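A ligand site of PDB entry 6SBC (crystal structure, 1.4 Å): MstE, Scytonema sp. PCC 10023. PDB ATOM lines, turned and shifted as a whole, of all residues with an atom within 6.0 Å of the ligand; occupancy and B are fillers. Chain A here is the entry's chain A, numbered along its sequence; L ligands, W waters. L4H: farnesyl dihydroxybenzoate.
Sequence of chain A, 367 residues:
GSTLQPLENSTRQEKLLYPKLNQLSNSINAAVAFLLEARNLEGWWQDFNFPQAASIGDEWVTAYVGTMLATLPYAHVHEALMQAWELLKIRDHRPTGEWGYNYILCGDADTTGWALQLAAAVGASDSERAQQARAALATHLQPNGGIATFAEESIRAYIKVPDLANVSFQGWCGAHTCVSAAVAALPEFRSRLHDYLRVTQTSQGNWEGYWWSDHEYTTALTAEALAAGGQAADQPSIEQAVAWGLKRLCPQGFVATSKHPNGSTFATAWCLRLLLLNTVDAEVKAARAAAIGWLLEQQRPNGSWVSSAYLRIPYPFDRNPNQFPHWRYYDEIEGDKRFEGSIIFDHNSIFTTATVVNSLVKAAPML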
ATOM      1  N   PHE A  50     -21.695  27.004   8.508  1.00  0.00           N
ATOM      2  CA  PHE A  50     -20.361  27.106   9.138  1.00  0.00           C
ATOM      3  C   PHE A  50     -19.355  26.935   8.026  1.00  0.00           C
ATOM      4  O   PHE A  50     -19.026  25.810   7.632  1.00  0.00           O
ATOM      5  CB  PHE A  50     -20.245  26.021  10.186  1.00  0.00           C
ATOM      6  CG  PHE A  50     -21.218  26.138  11.328  1.00  0.00           C
ATOM      7  CD1 PHE A  50     -22.431  25.482  11.308  1.00  0.00           C
ATOM      8  CD2 PHE A  50     -20.920  26.978  12.388  1.00  0.00           C
ATOM      9  CE1 PHE A  50     -23.334  25.665  12.331  1.00  0.00           C
ATOM     10  CE2 PHE A  50     -21.810  27.130  13.437  1.00  0.00           C
ATOM     11  CZ  PHE A  50     -23.011  26.473  13.400  1.00  0.00           C
ATOM     12  N   GLN A  52     -16.551  26.376   5.362  1.00  0.00           N
ATOM     13  CA  GLN A  52     -15.318  25.588   5.254  1.00  0.00           C
ATOM     14  C   GLN A  52     -15.254  24.643   6.445  1.00  0.00           C
ATOM     15  O   GLN A  52     -14.174  24.174   6.768  1.00  0.00           O
ATOM     16  CB  GLN A  52     -14.081  26.473   5.175  1.00  0.00           C
ATOM     17  CG  GLN A  52     -14.138  27.469   4.020  1.00  0.00           C
ATOM     18  CD  GLN A  52     -12.759  27.983   3.683  1.00  0.00           C
ATOM     19  OE1 GLN A  52     -12.168  28.785   4.413  1.00  0.00           O
ATOM     20  NE2 GLN A  52     -12.230  27.511   2.564  1.00  0.00           N
ATOM     21  N   ALA A  53     -16.380  24.333   7.062  1.00  0.00           N
ATOM     22  CA  ALA A  53     -16.360  23.487   8.245  1.00  0.00           C
ATOM     23  C   ALA A  53     -17.642  22.642   8.212  1.00  0.00           C
ATOM     24  O   ALA A  53     -17.870  21.964   7.206  1.00  0.00           O
ATOM     25  CB  ALA A  53     -16.224  24.390   9.427  1.00  0.00           C
ATOM     26  N   ALA A  54     -18.496  22.759   9.230  1.00  0.00           N
ATOM     27  CA  ALA A  54     -19.711  21.942   9.316  1.00  0.00           C
ATOM     28  C   ALA A  54     -20.662  22.235   8.154  1.00  0.00           C
ATOM     29  O   ALA A  54     -21.503  21.417   7.891  1.00  0.00           O
ATOM     30  CB  ALA A  54     -20.424  22.146  10.635  1.00  0.00           C
ATOM     31  N   SER A  55     -20.511  23.345   7.420  1.00  0.00           N
ATOM     32  CA  SER A  55     -21.322  23.587   6.205  1.00  0.00           C
ATOM     33  C   SER A  55     -22.770  23.835   6.614  1.00  0.00           C
ATOM     34  O   SER A  55     -23.032  24.480   7.666  1.00  0.00           O
ATOM     35  CB  SER A  55     -21.067  22.402   5.281  1.00  0.00           C
ATOM     36  OG  SER A  55     -21.856  22.335   4.160  1.00  0.00           O
ATOM     37  N   TRP A  60     -31.588  18.969  10.565  1.00  0.00           N
ATOM     38  CA  TRP A  60     -32.201  19.802  11.612  1.00  0.00           C
ATOM     39  C   TRP A  60     -33.206  20.818  11.035  1.00  0.00           C
ATOM     40  O   TRP A  60     -34.284  20.936  11.555  1.00  0.00           O
ATOM     41  CB  TRP A  60     -31.070  20.509  12.337  1.00  0.00           C
ATOM     42  CG  TRP A  60     -31.547  21.569  13.253  1.00  0.00           C
ATOM     43  CD1 TRP A  60     -32.524  21.517  14.191  1.00  0.00           C
ATOM     44  CD2 TRP A  60     -31.015  22.870  13.278  1.00  0.00           C
ATOM     45  NE1 TRP A  60     -32.674  22.741  14.777  1.00  0.00           N
ATOM     46  CE2 TRP A  60     -31.739  23.576  14.261  1.00  0.00           C
ATOM     47  CE3 TRP A  60     -30.042  23.542  12.527  1.00  0.00           C
ATOM     48  CZ2 TRP A  60     -31.460  24.900  14.573  1.00  0.00           C
ATOM     49  CZ3 TRP A  60     -29.738  24.836  12.872  1.00  0.00           C
ATOM     50  CH2 TRP A  60     -30.441  25.495  13.865  1.00  0.00           C
ATOM     51  N   GLY A 100     -28.779  14.608  13.168  1.00  0.00           N
ATOM     52  CA  GLY A 100     -27.855  15.679  13.495  1.00  0.00           C
ATOM     53  C   GLY A 100     -28.025  16.883  12.578  1.00  0.00           C
ATOM     54  O   GLY A 100     -28.946  16.951  11.766  1.00  0.00           O
ATOM     55  N   TYR A 101     -27.126  17.839  12.729  1.00  0.00           N
ATOM     56  CA  TYR A 101     -27.246  19.098  12.015  1.00  0.00           C
ATOM     57  C   TYR A 101     -27.308  18.848  10.513  1.00  0.00           C
ATOM     58  O   TYR A 101     -28.165  19.431   9.815  1.00  0.00           O
ATOM     59  CB  TYR A 101     -26.033  19.956  12.393  1.00  0.00           C
ATOM     60  CG  TYR A 101     -25.828  21.229  11.614  1.00  0.00           C
ATOM     61  CD1 TYR A 101     -24.843  21.328  10.638  1.00  0.00           C
ATOM     62  CD2 TYR A 101     -26.570  22.355  11.871  1.00  0.00           C
ATOM     63  CE1 TYR A 101     -24.644  22.489   9.919  1.00  0.00           C
ATOM     64  CE2 TYR A 101     -26.416  23.522  11.118  1.00  0.00           C
ATOM     65  CZ  TYR A 101     -25.440  23.601  10.138  1.00  0.00           C
ATOM     66  OH  TYR A 101     -25.186  24.784   9.469  1.00  0.00           O
ATOM     67  N   LEU A 105     -22.315  15.629  10.658  1.00  0.00           N
ATOM     68  CA  LEU A 105     -22.333  15.811  12.123  1.00  0.00           C
ATOM     69  C   LEU A 105     -22.786  14.544  12.808  1.00  0.00           C
ATOM     70  O   LEU A 105     -23.512  13.759  12.251  1.00  0.00           O
ATOM     71  CB  LEU A 105     -23.203  16.996  12.552  1.00  0.00           C
ATOM     72  CG  LEU A 105     -22.417  18.240  12.942  1.00  0.00           C
ATOM     73  CD1 LEU A 105     -21.599  18.048  14.193  1.00  0.00           C
ATOM     74  CD2 LEU A 105     -21.554  18.711  11.790  1.00  0.00           C
ATOM     75  N   ASP A 108     -27.509  14.634  17.560  1.00  0.00           N
ATOM     76  CA  ASP A 108     -27.776  15.567  18.670  1.00  0.00           C
ATOM     77  C   ASP A 108     -29.238  15.482  19.076  1.00  0.00           C
ATOM     78  O   ASP A 108     -30.090  15.110  18.261  1.00  0.00           O
ATOM     79  CB  ASP A 108     -27.302  16.976  18.353  1.00  0.00           C
ATOM     80  CG  ASP A 108     -28.297  17.712  17.498  1.00  0.00           C
ATOM     81  OD1 ASP A 108     -28.036  17.706  16.272  1.00  0.00           O
ATOM     82  OD2 ASP A 108     -29.266  18.293  18.060  1.00  0.00           O
ATOM     83  N   ASP A 110     -31.300  17.886  19.920  1.00  0.00           N
ATOM     84  CA  ASP A 110     -32.228  18.921  19.408  1.00  0.00           C
ATOM     85  C   ASP A 110     -32.787  18.485  18.056  1.00  0.00           C
ATOM     86  O   ASP A 110     -34.018  18.428  17.856  1.00  0.00           O
ATOM     87  CB  ASP A 110     -31.579  20.289  19.385  1.00  0.00           C
ATOM     88  CG  ASP A 110     -32.650  21.338  19.165  1.00  0.00           C
ATOM     89  OD1 ASP A 110     -33.652  21.336  19.918  1.00  0.00           O
ATOM     90  OD2 ASP A 110     -32.469  22.125  18.260  1.00  0.00           O
ATOM     91  N   THR A 111     -31.904  18.143  17.114  1.00  0.00           N
ATOM     92  CA  THR A 111     -32.374  17.687  15.817  1.00  0.00           C
ATOM     93  C   THR A 111     -33.304  16.487  15.999  1.00  0.00           C
ATOM     94  O   THR A 111     -34.336  16.374  15.329  1.00  0.00           O
ATOM     95  CB  THR A 111     -31.191  17.287  14.914  1.00  0.00           C
ATOM     96  OG1 THR A 111     -30.305  18.396  14.799  1.00  0.00           O
ATOM     97  CG2 THR A 111     -31.659  16.802  13.584  1.00  0.00           C
ATOM     98  N   THR A 149     -27.420  18.528  24.530  1.00  0.00           N
ATOM     99  CA  THR A 149     -27.423  18.441  23.050  1.00  0.00           C
ATOM    100  C   THR A 149     -26.574  17.258  22.555  1.00  0.00           C
ATOM    101  O   THR A 149     -27.022  16.460  21.704  1.00  0.00           O
ATOM    102  CB  THR A 149     -26.938  19.770  22.441  1.00  0.00           C
ATOM    103  OG1 THR A 149     -27.838  20.794  22.845  1.00  0.00           O
ATOM    104  CG2 THR A 149     -26.847  19.718  20.924  1.00  0.00           C
ATOM    105  N   PHE A 150     -25.343  17.200  23.057  1.00  0.00           N
ATOM    106  CA  PHE A 150     -24.351  16.265  22.509  1.00  0.00           C
ATOM    107  C   PHE A 150     -23.876  15.283  23.567  1.00  0.00           C
ATOM    108  O   PHE A 150     -23.776  15.670  24.743  1.00  0.00           O
ATOM    109  CB  PHE A 150     -23.124  17.035  22.028  1.00  0.00           C
ATOM    110  CG  PHE A 150     -23.338  17.829  20.774  1.00  0.00           C
ATOM    111  CD1 PHE A 150     -23.185  19.201  20.776  1.00  0.00           C
ATOM    112  CD2 PHE A 150     -23.660  17.205  19.593  1.00  0.00           C
ATOM    113  CE1 PHE A 150     -23.355  19.949  19.621  1.00  0.00           C
ATOM    114  CE2 PHE A 150     -23.785  17.938  18.436  1.00  0.00           C
ATOM    115  CZ  PHE A 150     -23.656  19.315  18.470  1.00  0.00           C
ATOM    116  N   ILE A 155     -19.163  14.321  19.893  1.00  0.00           N
ATOM    117  CA  ILE A 155     -18.820  15.651  19.368  1.00  0.00           C
ATOM    118  C   ILE A 155     -17.311  15.905  19.395  1.00  0.00           C
ATOM    119  O   ILE A 155     -16.812  16.472  18.476  1.00  0.00           O
ATOM    120  CB  ILE A 155     -19.649  16.750  20.036  1.00  0.00           C
ATOM    121  CG1 ILE A 155     -19.556  18.106  19.339  1.00  0.00           C
ATOM    122  CG2 ILE A 155     -19.354  16.914  21.507  1.00  0.00           C
ATOM    123  CD1 ILE A 155     -19.959  18.115  17.855  1.00  0.00           C
ATOM    124  N   TYR A 158     -15.889  14.520  16.288  1.00  0.00           N
ATOM    125  CA  TYR A 158     -16.223  15.298  15.086  1.00  0.00           C
ATOM    126  C   TYR A 158     -15.251  16.481  15.011  1.00  0.00           C
ATOM    127  O   TYR A 158     -14.721  16.767  13.929  1.00  0.00           O
ATOM    128  CB  TYR A 158     -17.674  15.787  15.100  1.00  0.00           C
ATOM    129  CG  TYR A 158     -17.845  16.816  14.008  1.00  0.00           C
ATOM    130  CD1 TYR A 158     -17.788  18.166  14.303  1.00  0.00           C
ATOM    131  CD2 TYR A 158     -17.920  16.458  12.673  1.00  0.00           C
ATOM    132  CE1 TYR A 158     -17.878  19.121  13.316  1.00  0.00           C
ATOM    133  CE2 TYR A 158     -18.028  17.407  11.673  1.00  0.00           C
ATOM    134  CZ  TYR A 158     -17.920  18.751  11.994  1.00  0.00           C
ATOM    135  OH  TYR A 158     -17.945  19.674  10.996  1.00  0.00           O
ATOM    136  N   ILE A 159     -15.071  17.161  16.143  1.00  0.00           N
ATOM    137  CA  ILE A 159     -14.288  18.426  16.206  1.00  0.00           C
ATOM    138  C   ILE A 159     -12.791  18.111  16.040  1.00  0.00           C
ATOM    139  O   ILE A 159     -12.267  17.206  16.726  1.00  0.00           O
ATOM    140  CB  ILE A 159     -14.558  19.172  17.538  1.00  0.00           C
ATOM    141  CG1 ILE A 159     -15.984  19.717  17.625  1.00  0.00           C
ATOM    142  CG2 ILE A 159     -13.564  20.302  17.783  1.00  0.00           C
ATOM    143  CD1 ILE A 159     -16.332  20.825  16.678  1.00  0.00           C
ATOM    144  N   LYS A 160     -12.125  18.862  15.156  1.00  0.00           N
ATOM    145  CA  LYS A 160     -10.685  18.610  14.841  1.00  0.00           C
ATOM    146  C   LYS A 160      -9.875  19.891  14.883  1.00  0.00           C
ATOM    147  O   LYS A 160      -8.981  20.065  14.042  1.00  0.00           O
ATOM    148  CB  LYS A 160     -10.544  17.826  13.533  1.00  0.00           C
ATOM    149  CG  LYS A 160     -11.101  16.426  13.701  1.00  0.00           C
ATOM    150  CD  LYS A 160     -11.014  15.498  12.560  1.00  0.00           C
ATOM    151  CE  LYS A 160     -11.861  14.281  12.878  1.00  0.00           C
ATOM    152  NZ  LYS A 160     -11.655  13.196  11.906  1.00  0.00           N
ATOM    153  N   VAL A 161     -10.152  20.709  15.890  1.00  0.00           N
ATOM    154  CA  VAL A 161      -9.546  22.053  16.075  1.00  0.00           C
ATOM    155  C   VAL A 161      -8.478  21.905  17.141  1.00  0.00           C
ATOM    156  O   VAL A 161      -8.836  21.529  18.273  1.00  0.00           O
ATOM    157  CB  VAL A 161     -10.630  23.056  16.498  1.00  0.00           C
ATOM    158  CG1 VAL A 161     -10.066  24.445  16.807  1.00  0.00           C
ATOM    159  CG2 VAL A 161     -11.742  23.104  15.463  1.00  0.00           C
ATOM    160  N   LEU A 164      -8.882  23.180  20.788  1.00  0.00           N
ATOM    161  CA  LEU A 164     -10.010  22.567  21.556  1.00  0.00           C
ATOM    162  C   LEU A 164      -9.717  21.094  21.915  1.00  0.00           C
ATOM    163  O   LEU A 164     -10.582  20.468  22.565  1.00  0.00           O
ATOM    164  CB  LEU A 164     -11.313  22.692  20.770  1.00  0.00           C
ATOM    165  CG  LEU A 164     -11.728  24.125  20.378  1.00  0.00           C
ATOM    166  CD1 LEU A 164     -12.982  24.141  19.505  1.00  0.00           C
ATOM    167  CD2 LEU A 164     -11.933  24.981  21.630  1.00  0.00           C
ATOM    168  N   TRP A 172     -21.164  22.203  25.960  1.00  0.00           N
ATOM    169  CA  TRP A 172     -21.932  21.576  24.879  1.00  0.00           C
ATOM    170  C   TRP A 172     -22.646  20.292  25.304  1.00  0.00           C
ATOM    171  O   TRP A 172     -23.586  19.893  24.602  1.00  0.00           O
ATOM    172  CB  TRP A 172     -21.019  21.288  23.704  1.00  0.00           C
ATOM    173  CG  TRP A 172     -20.536  22.514  22.983  1.00  0.00           C
ATOM    174  CD1 TRP A 172     -20.740  23.846  23.267  1.00  0.00           C
ATOM    175  CD2 TRP A 172     -19.805  22.488  21.753  1.00  0.00           C
ATOM    176  NE1 TRP A 172     -20.114  24.630  22.323  1.00  0.00           N
ATOM    177  CE2 TRP A 172     -19.568  23.830  21.361  1.00  0.00           C
ATOM    178  CE3 TRP A 172     -19.354  21.456  20.938  1.00  0.00           C
ATOM    179  CZ2 TRP A 172     -18.868  24.147  20.198  1.00  0.00           C
ATOM    180  CZ3 TRP A 172     -18.666  21.775  19.792  1.00  0.00           C
ATOM    181  CH2 TRP A 172     -18.448  23.106  19.424  1.00  0.00           C
ATOM    182  N   VAL A 179     -33.164  22.924  24.306  1.00  0.00           N
ATOM    183  CA  VAL A 179     -33.340  21.564  23.776  1.00  0.00           C
ATOM    184  C   VAL A 179     -34.301  20.794  24.686  1.00  0.00           C
ATOM    185  O   VAL A 179     -35.128  20.040  24.200  1.00  0.00           O
ATOM    186  CB  VAL A 179     -31.966  20.898  23.692  1.00  0.00           C
ATOM    187  CG1 VAL A 179     -32.136  19.501  23.160  1.00  0.00           C
ATOM    188  CG2 VAL A 179     -30.986  21.724  22.839  1.00  0.00           C
ATOM    189  N   TRP A 211     -28.208  27.738  22.867  1.00  0.00           N
ATOM    190  CA  TRP A 211     -27.765  27.987  21.466  1.00  0.00           C
ATOM    191  C   TRP A 211     -28.444  29.225  20.847  1.00  0.00           C
ATOM    192  O   TRP A 211     -28.090  29.581  19.752  1.00  0.00           O
ATOM    193  CB  TRP A 211     -28.059  26.765  20.596  1.00  0.00           C
ATOM    194  CG  TRP A 211     -27.393  25.496  21.037  1.00  0.00           C
ATOM    195  CD1 TRP A 211     -28.055  24.458  21.590  1.00  0.00           C
ATOM    196  CD2 TRP A 211     -26.022  25.123  20.900  1.00  0.00           C
ATOM    197  NE1 TRP A 211     -27.164  23.458  21.859  1.00  0.00           N
ATOM    198  CE2 TRP A 211     -25.927  23.834  21.426  1.00  0.00           C
ATOM    199  CE3 TRP A 211     -24.854  25.730  20.447  1.00  0.00           C
ATOM    200  CZ2 TRP A 211     -24.706  23.145  21.508  1.00  0.00           C
ATOM    201  CZ3 TRP A 211     -23.667  25.046  20.504  1.00  0.00           C
ATOM    202  CH2 TRP A 211     -23.575  23.772  21.038  1.00  0.00           C
ATOM    203  N   LEU A 311     -28.343  31.976  15.897  1.00  0.00           N
ATOM    204  CA  LEU A 311     -27.735  30.763  16.498  1.00  0.00           C
ATOM    205  C   LEU A 311     -26.338  31.108  16.967  1.00  0.00           C
ATOM    206  O   LEU A 311     -25.529  31.576  16.186  1.00  0.00           O
ATOM    207  CB  LEU A 311     -27.721  29.668  15.438  1.00  0.00           C
ATOM    208  CG  LEU A 311     -27.264  28.287  15.853  1.00  0.00           C
ATOM    209  CD1 LEU A 311     -28.246  27.658  16.828  1.00  0.00           C
ATOM    210  CD2 LEU A 311     -27.137  27.422  14.621  1.00  0.00           C
ATOM    211  N   ARG A 312     -26.108  30.934  18.249  1.00  0.00           N
ATOM    212  CA  ARG A 312     -24.769  31.248  18.791  1.00  0.00           C
ATOM    213  C   ARG A 312     -24.008  29.985  19.188  1.00  0.00           C
ATOM    214  O   ARG A 312     -24.632  28.988  19.615  1.00  0.00           O
ATOM    215  CB  ARG A 312     -24.891  32.182  19.957  1.00  0.00           C
ATOM    216  CG  ARG A 312     -25.547  31.573  21.152  1.00  0.00           C
ATOM    217  CD  ARG A 312     -26.054  32.638  22.084  1.00  0.00           C
ATOM    218  NE  ARG A 312     -26.611  32.029  23.265  1.00  0.00           N
ATOM    219  CZ  ARG A 312     -27.155  32.694  24.284  1.00  0.00           C
ATOM    220  NH1 ARG A 312     -27.692  31.998  25.267  1.00  0.00           N
ATOM    221  NH2 ARG A 312     -27.167  34.019  24.285  1.00  0.00           N
ATOM    222  N   ILE A 313     -22.690  30.122  19.118  1.00  0.00           N
ATOM    223  CA  ILE A 313     -21.802  28.988  19.427  1.00  0.00           C
ATOM    224  C   ILE A 313     -20.986  29.368  20.638  1.00  0.00           C
ATOM    225  O   ILE A 313     -19.967  30.034  20.517  1.00  0.00           O
ATOM    226  CB  ILE A 313     -20.902  28.616  18.254  1.00  0.00           C
ATOM    227  CG1 ILE A 313     -21.702  28.339  16.980  1.00  0.00           C
ATOM    228  CG2 ILE A 313     -20.044  27.402  18.590  1.00  0.00           C
ATOM    229  CD1 ILE A 313     -22.682  27.179  17.033  1.00  0.00           C
ATOM    230  N   PRO A 314     -21.385  28.921  21.849  1.00  0.00           N
ATOM    231  CA  PRO A 314     -20.536  29.123  23.008  1.00  0.00           C
ATOM    232  C   PRO A 314     -19.238  28.331  22.849  1.00  0.00           C
ATOM    233  O   PRO A 314     -19.209  27.309  22.174  1.00  0.00           O
ATOM    234  CB  PRO A 314     -21.392  28.623  24.194  1.00  0.00           C
ATOM    235  CG  PRO A 314     -22.812  28.544  23.648  1.00  0.00           C
ATOM    236  CD  PRO A 314     -22.564  28.148  22.204  1.00  0.00           C
ATOM    237  N   ARG A 338     -13.312  32.828  14.506  1.00  0.00           N
ATOM    238  CA  ARG A 338     -13.663  31.466  14.869  1.00  0.00           C
ATOM    239  C   ARG A 338     -15.147  31.452  15.149  1.00  0.00           C
ATOM    240  O   ARG A 338     -15.764  32.508  15.357  1.00  0.00           O
ATOM    241  CB  ARG A 338     -12.771  30.975  16.014  1.00  0.00           C
ATOM    242  CG  ARG A 338     -13.105  31.566  17.370  1.00  0.00           C
ATOM    243  CD  ARG A 338     -12.137  31.068  18.423  1.00  0.00           C
ATOM    244  NE  ARG A 338     -12.160  29.602  18.552  1.00  0.00           N
ATOM    245  CZ  ARG A 338     -11.176  28.866  19.052  1.00  0.00           C
ATOM    246  NH1 ARG A 338     -10.107  29.441  19.587  1.00  0.00           N
ATOM    247  NH2 ARG A 338     -11.275  27.536  19.046  1.00  0.00           N
ATOM    248  N   PHE A 339     -15.705  30.272  15.226  1.00  0.00           N
ATOM    249  CA  PHE A 339     -17.145  30.123  15.495  1.00  0.00           C
ATOM    250  C   PHE A 339     -17.468  30.408  16.961  1.00  0.00           C
ATOM    251  O   PHE A 339     -18.510  30.945  17.315  1.00  0.00           O
ATOM    252  CB  PHE A 339     -17.660  28.738  15.096  1.00  0.00           C
ATOM    253  CG  PHE A 339     -17.543  28.476  13.614  1.00  0.00           C
ATOM    254  CD1 PHE A 339     -16.871  27.363  13.156  1.00  0.00           C
ATOM    255  CD2 PHE A 339     -18.020  29.382  12.676  1.00  0.00           C
ATOM    256  CE1 PHE A 339     -16.699  27.132  11.809  1.00  0.00           C
ATOM    257  CE2 PHE A 339     -17.873  29.140  11.312  1.00  0.00           C
ATOM    258  CZ  PHE A 339     -17.215  28.023  10.883  1.00  0.00           C
ATOM    259  N   GLU A 340     -16.578  29.953  17.853  1.00  0.00           N
ATOM    260  CA  GLU A 340     -16.812  30.131  19.286  1.00  0.00           C
ATOM    261  C   GLU A 340     -16.879  31.638  19.620  1.00  0.00           C
ATOM    262  O   GLU A 340     -15.992  32.411  19.253  1.00  0.00           O
ATOM    263  CB  GLU A 340     -15.710  29.522  20.115  1.00  0.00           C
ATOM    264  CG  GLU A 340     -15.661  28.004  20.055  1.00  0.00           C
ATOM    265  CD  GLU A 340     -15.112  27.382  18.785  1.00  0.00           C
ATOM    266  OE1 GLU A 340     -15.475  26.172  18.560  1.00  0.00           O
ATOM    267  OE2 GLU A 340     -14.324  28.060  18.011  1.00  0.00           O
HETATM  268  C6  L4H L   1     -17.904  23.543  14.098  1.00  0.00           C
HETATM  269  C7  L4H L   1     -18.243  24.301  15.204  1.00  0.00           C
HETATM  270  C8  L4H L   1     -19.617  24.610  15.596  1.00  0.00           C
HETATM  271  C10 L4H L   1     -21.101  22.604  14.889  1.00  0.00           C
HETATM  272  C13 L4H L   1     -24.214  22.801  14.969  1.00  0.00           C
HETATM  273  C15 L4H L   1     -25.341  24.561  16.526  1.00  0.00           C
HETATM  274  C17 L4H L   1     -27.529  23.420  16.398  1.00  0.00           C
HETATM  275  C20 L4H L   1     -28.944  21.300  15.806  1.00  0.00           C
HETATM  276  C21 L4H L   1     -23.534  22.968  17.413  1.00  0.00           C
HETATM  277  C22 L4H L   1     -20.365  21.666  15.820  1.00  0.00           C
HETATM  278  C18 L4H L   1     -28.008  22.099  16.762  1.00  0.00           C
HETATM  279  C19 L4H L   1     -27.627  21.567  18.101  1.00  0.00           C
HETATM  280  C16 L4H L   1     -26.565  24.085  17.317  1.00  0.00           C
HETATM  281  C14 L4H L   1     -24.422  23.374  16.319  1.00  0.00           C
HETATM  282  C12 L4H L   1     -23.382  21.655  14.743  1.00  0.00           C
HETATM  283  C11 L4H L   1     -22.159  22.045  13.937  1.00  0.00           C
HETATM  284  C9  L4H L   1     -20.704  23.994  14.780  1.00  0.00           C
HETATM  285  C2  L4H L   1     -16.561  23.260  13.717  1.00  0.00           C
HETATM  286  C3  L4H L   1     -16.284  22.467  12.546  1.00  0.00           C
HETATM  287  O4  L4H L   1     -15.067  22.170  12.225  1.00  0.00           O
HETATM  288  O5  L4H L   1     -17.228  22.033  11.809  1.00  0.00           O
HETATM  289  C1  L4H L   1     -15.530  23.812  14.502  1.00  0.00           C
HETATM  290  C25 L4H L   1     -15.850  24.581  15.607  1.00  0.00           C
HETATM  291  O26 L4H L   1     -14.790  25.015  16.404  1.00  0.00           O
HETATM  292  C23 L4H L   1     -17.183  24.812  15.978  1.00  0.00           C
HETATM  293  O24 L4H L   1     -17.496  25.551  17.068  1.00  0.00           O
HETATM  294  O   HOH W   1     -30.034  23.912  18.492  1.00  0.00           O
HETATM  295  O   HOH W   2     -12.993  23.992  11.732  1.00  0.00           O
HETATM  296  O   HOH W   3     -14.367  21.082   9.810  1.00  0.00           O
HETATM  297  O   HOH W   4     -14.092  27.759  15.053  1.00  0.00           O
HETATM  298  O   HOH W   5     -13.454  20.254  13.089  1.00  0.00           O
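O of Phe 50 is in hydrogen-bond range of N of Ser 55, at 2.9 Å.
OG1 of Thr 111 is in hydrogen-bond range of OD1 of Asp 108.
OH of Tyr 101 is in hydrogen-bond range of O of Ser 55, at 2.8 Å.
The indole nitrogen of Trp 172 is in hydrogen-bond range of the backbone carbonyl oxygen of Pro 314.
OD2 of Asp 108 lies within hydrogen-bond range of N of Asp 110 (2.8 Å).
N of Arg 312 is in hydrogen-bond range of O of Trp 211, 2.8 Å away.
NE of Arg 338 lies within salt-bridge range of OE2 of Glu 340 (2.7 Å).
The indole nitrogen (NE1) of Trp 211 lies within hydrogen-bond range of the side-chain hydroxyl (OG1) of Thr 149 (2.9 Å).
Water W5 bridges O4 of the ligand (2.6 Å) and N of Lys 160 (2.8 Å).
Water W4 lies within hydrogen-bond range of the side-chain carboxylate of Glu 340 (3.0 Å), the backbone NH of Phe 339 (3.0 Å) and an oxygen (O26) of the ligand (3.1 Å).
The backbone NH (N) of Ala 54 sits at hydrogen-bond distance from an oxygen (O5) of the ligand, at 3.0 Å.
An oxygen (O26) of the ligand lies within hydrogen-bond range of the side-chain carboxylate (OE1) of Glu 340 (2.5 Å).
An oxygen (O5) of the ligand lies within hydrogen-bond range of the side-chain hydroxyl (OH) of Tyr 158 (2.6 Å).
Residues that only touch the ligand: Phe 50 (3.6 Å), Ala 53 (3.5 Å), Trp 60 (3.6 Å), Tyr 101 (3.9 Å), Leu 105 (3.9 Å), Asp 108 (3.7 Å), Thr 111 (3.4 Å), Thr 149 (3.5 Å), Phe 150 (3.7 Å), Ile 159 (3.8 Å), Val 161 (3.7 Å), Leu 164 (3.7 Å), Trp 172 (3.5 Å), Trp 211 (3.7 Å), Leu 311 (3.9 Å), Ile 313 (3.5 Å) and Phe 339 (3.8 Å).
Hydrophobic or aromatic side chains within 4 Å of the ligand: Phe 50, Ala 53, Ala 54, Trp 60, Tyr 101, Leu 105, Phe 150, Tyr 158, Ile 159, Val 161, Leu 164, Trp 172, Trp 211, Leu 311, Ile 313 and Phe 339.
20 residues have an atom within 4 Å of the ligand: Phe 50, Ala 53, Ala 54, Trp 60, Tyr 101, Leu 105, Asp 108, Thr 111, Thr 149, Phe 150, Tyr 158, Ile 159, Val 161, Leu 164, Trp 172, Trp 211, Leu 311, Ile 313, Phe 339 and Glu 340.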
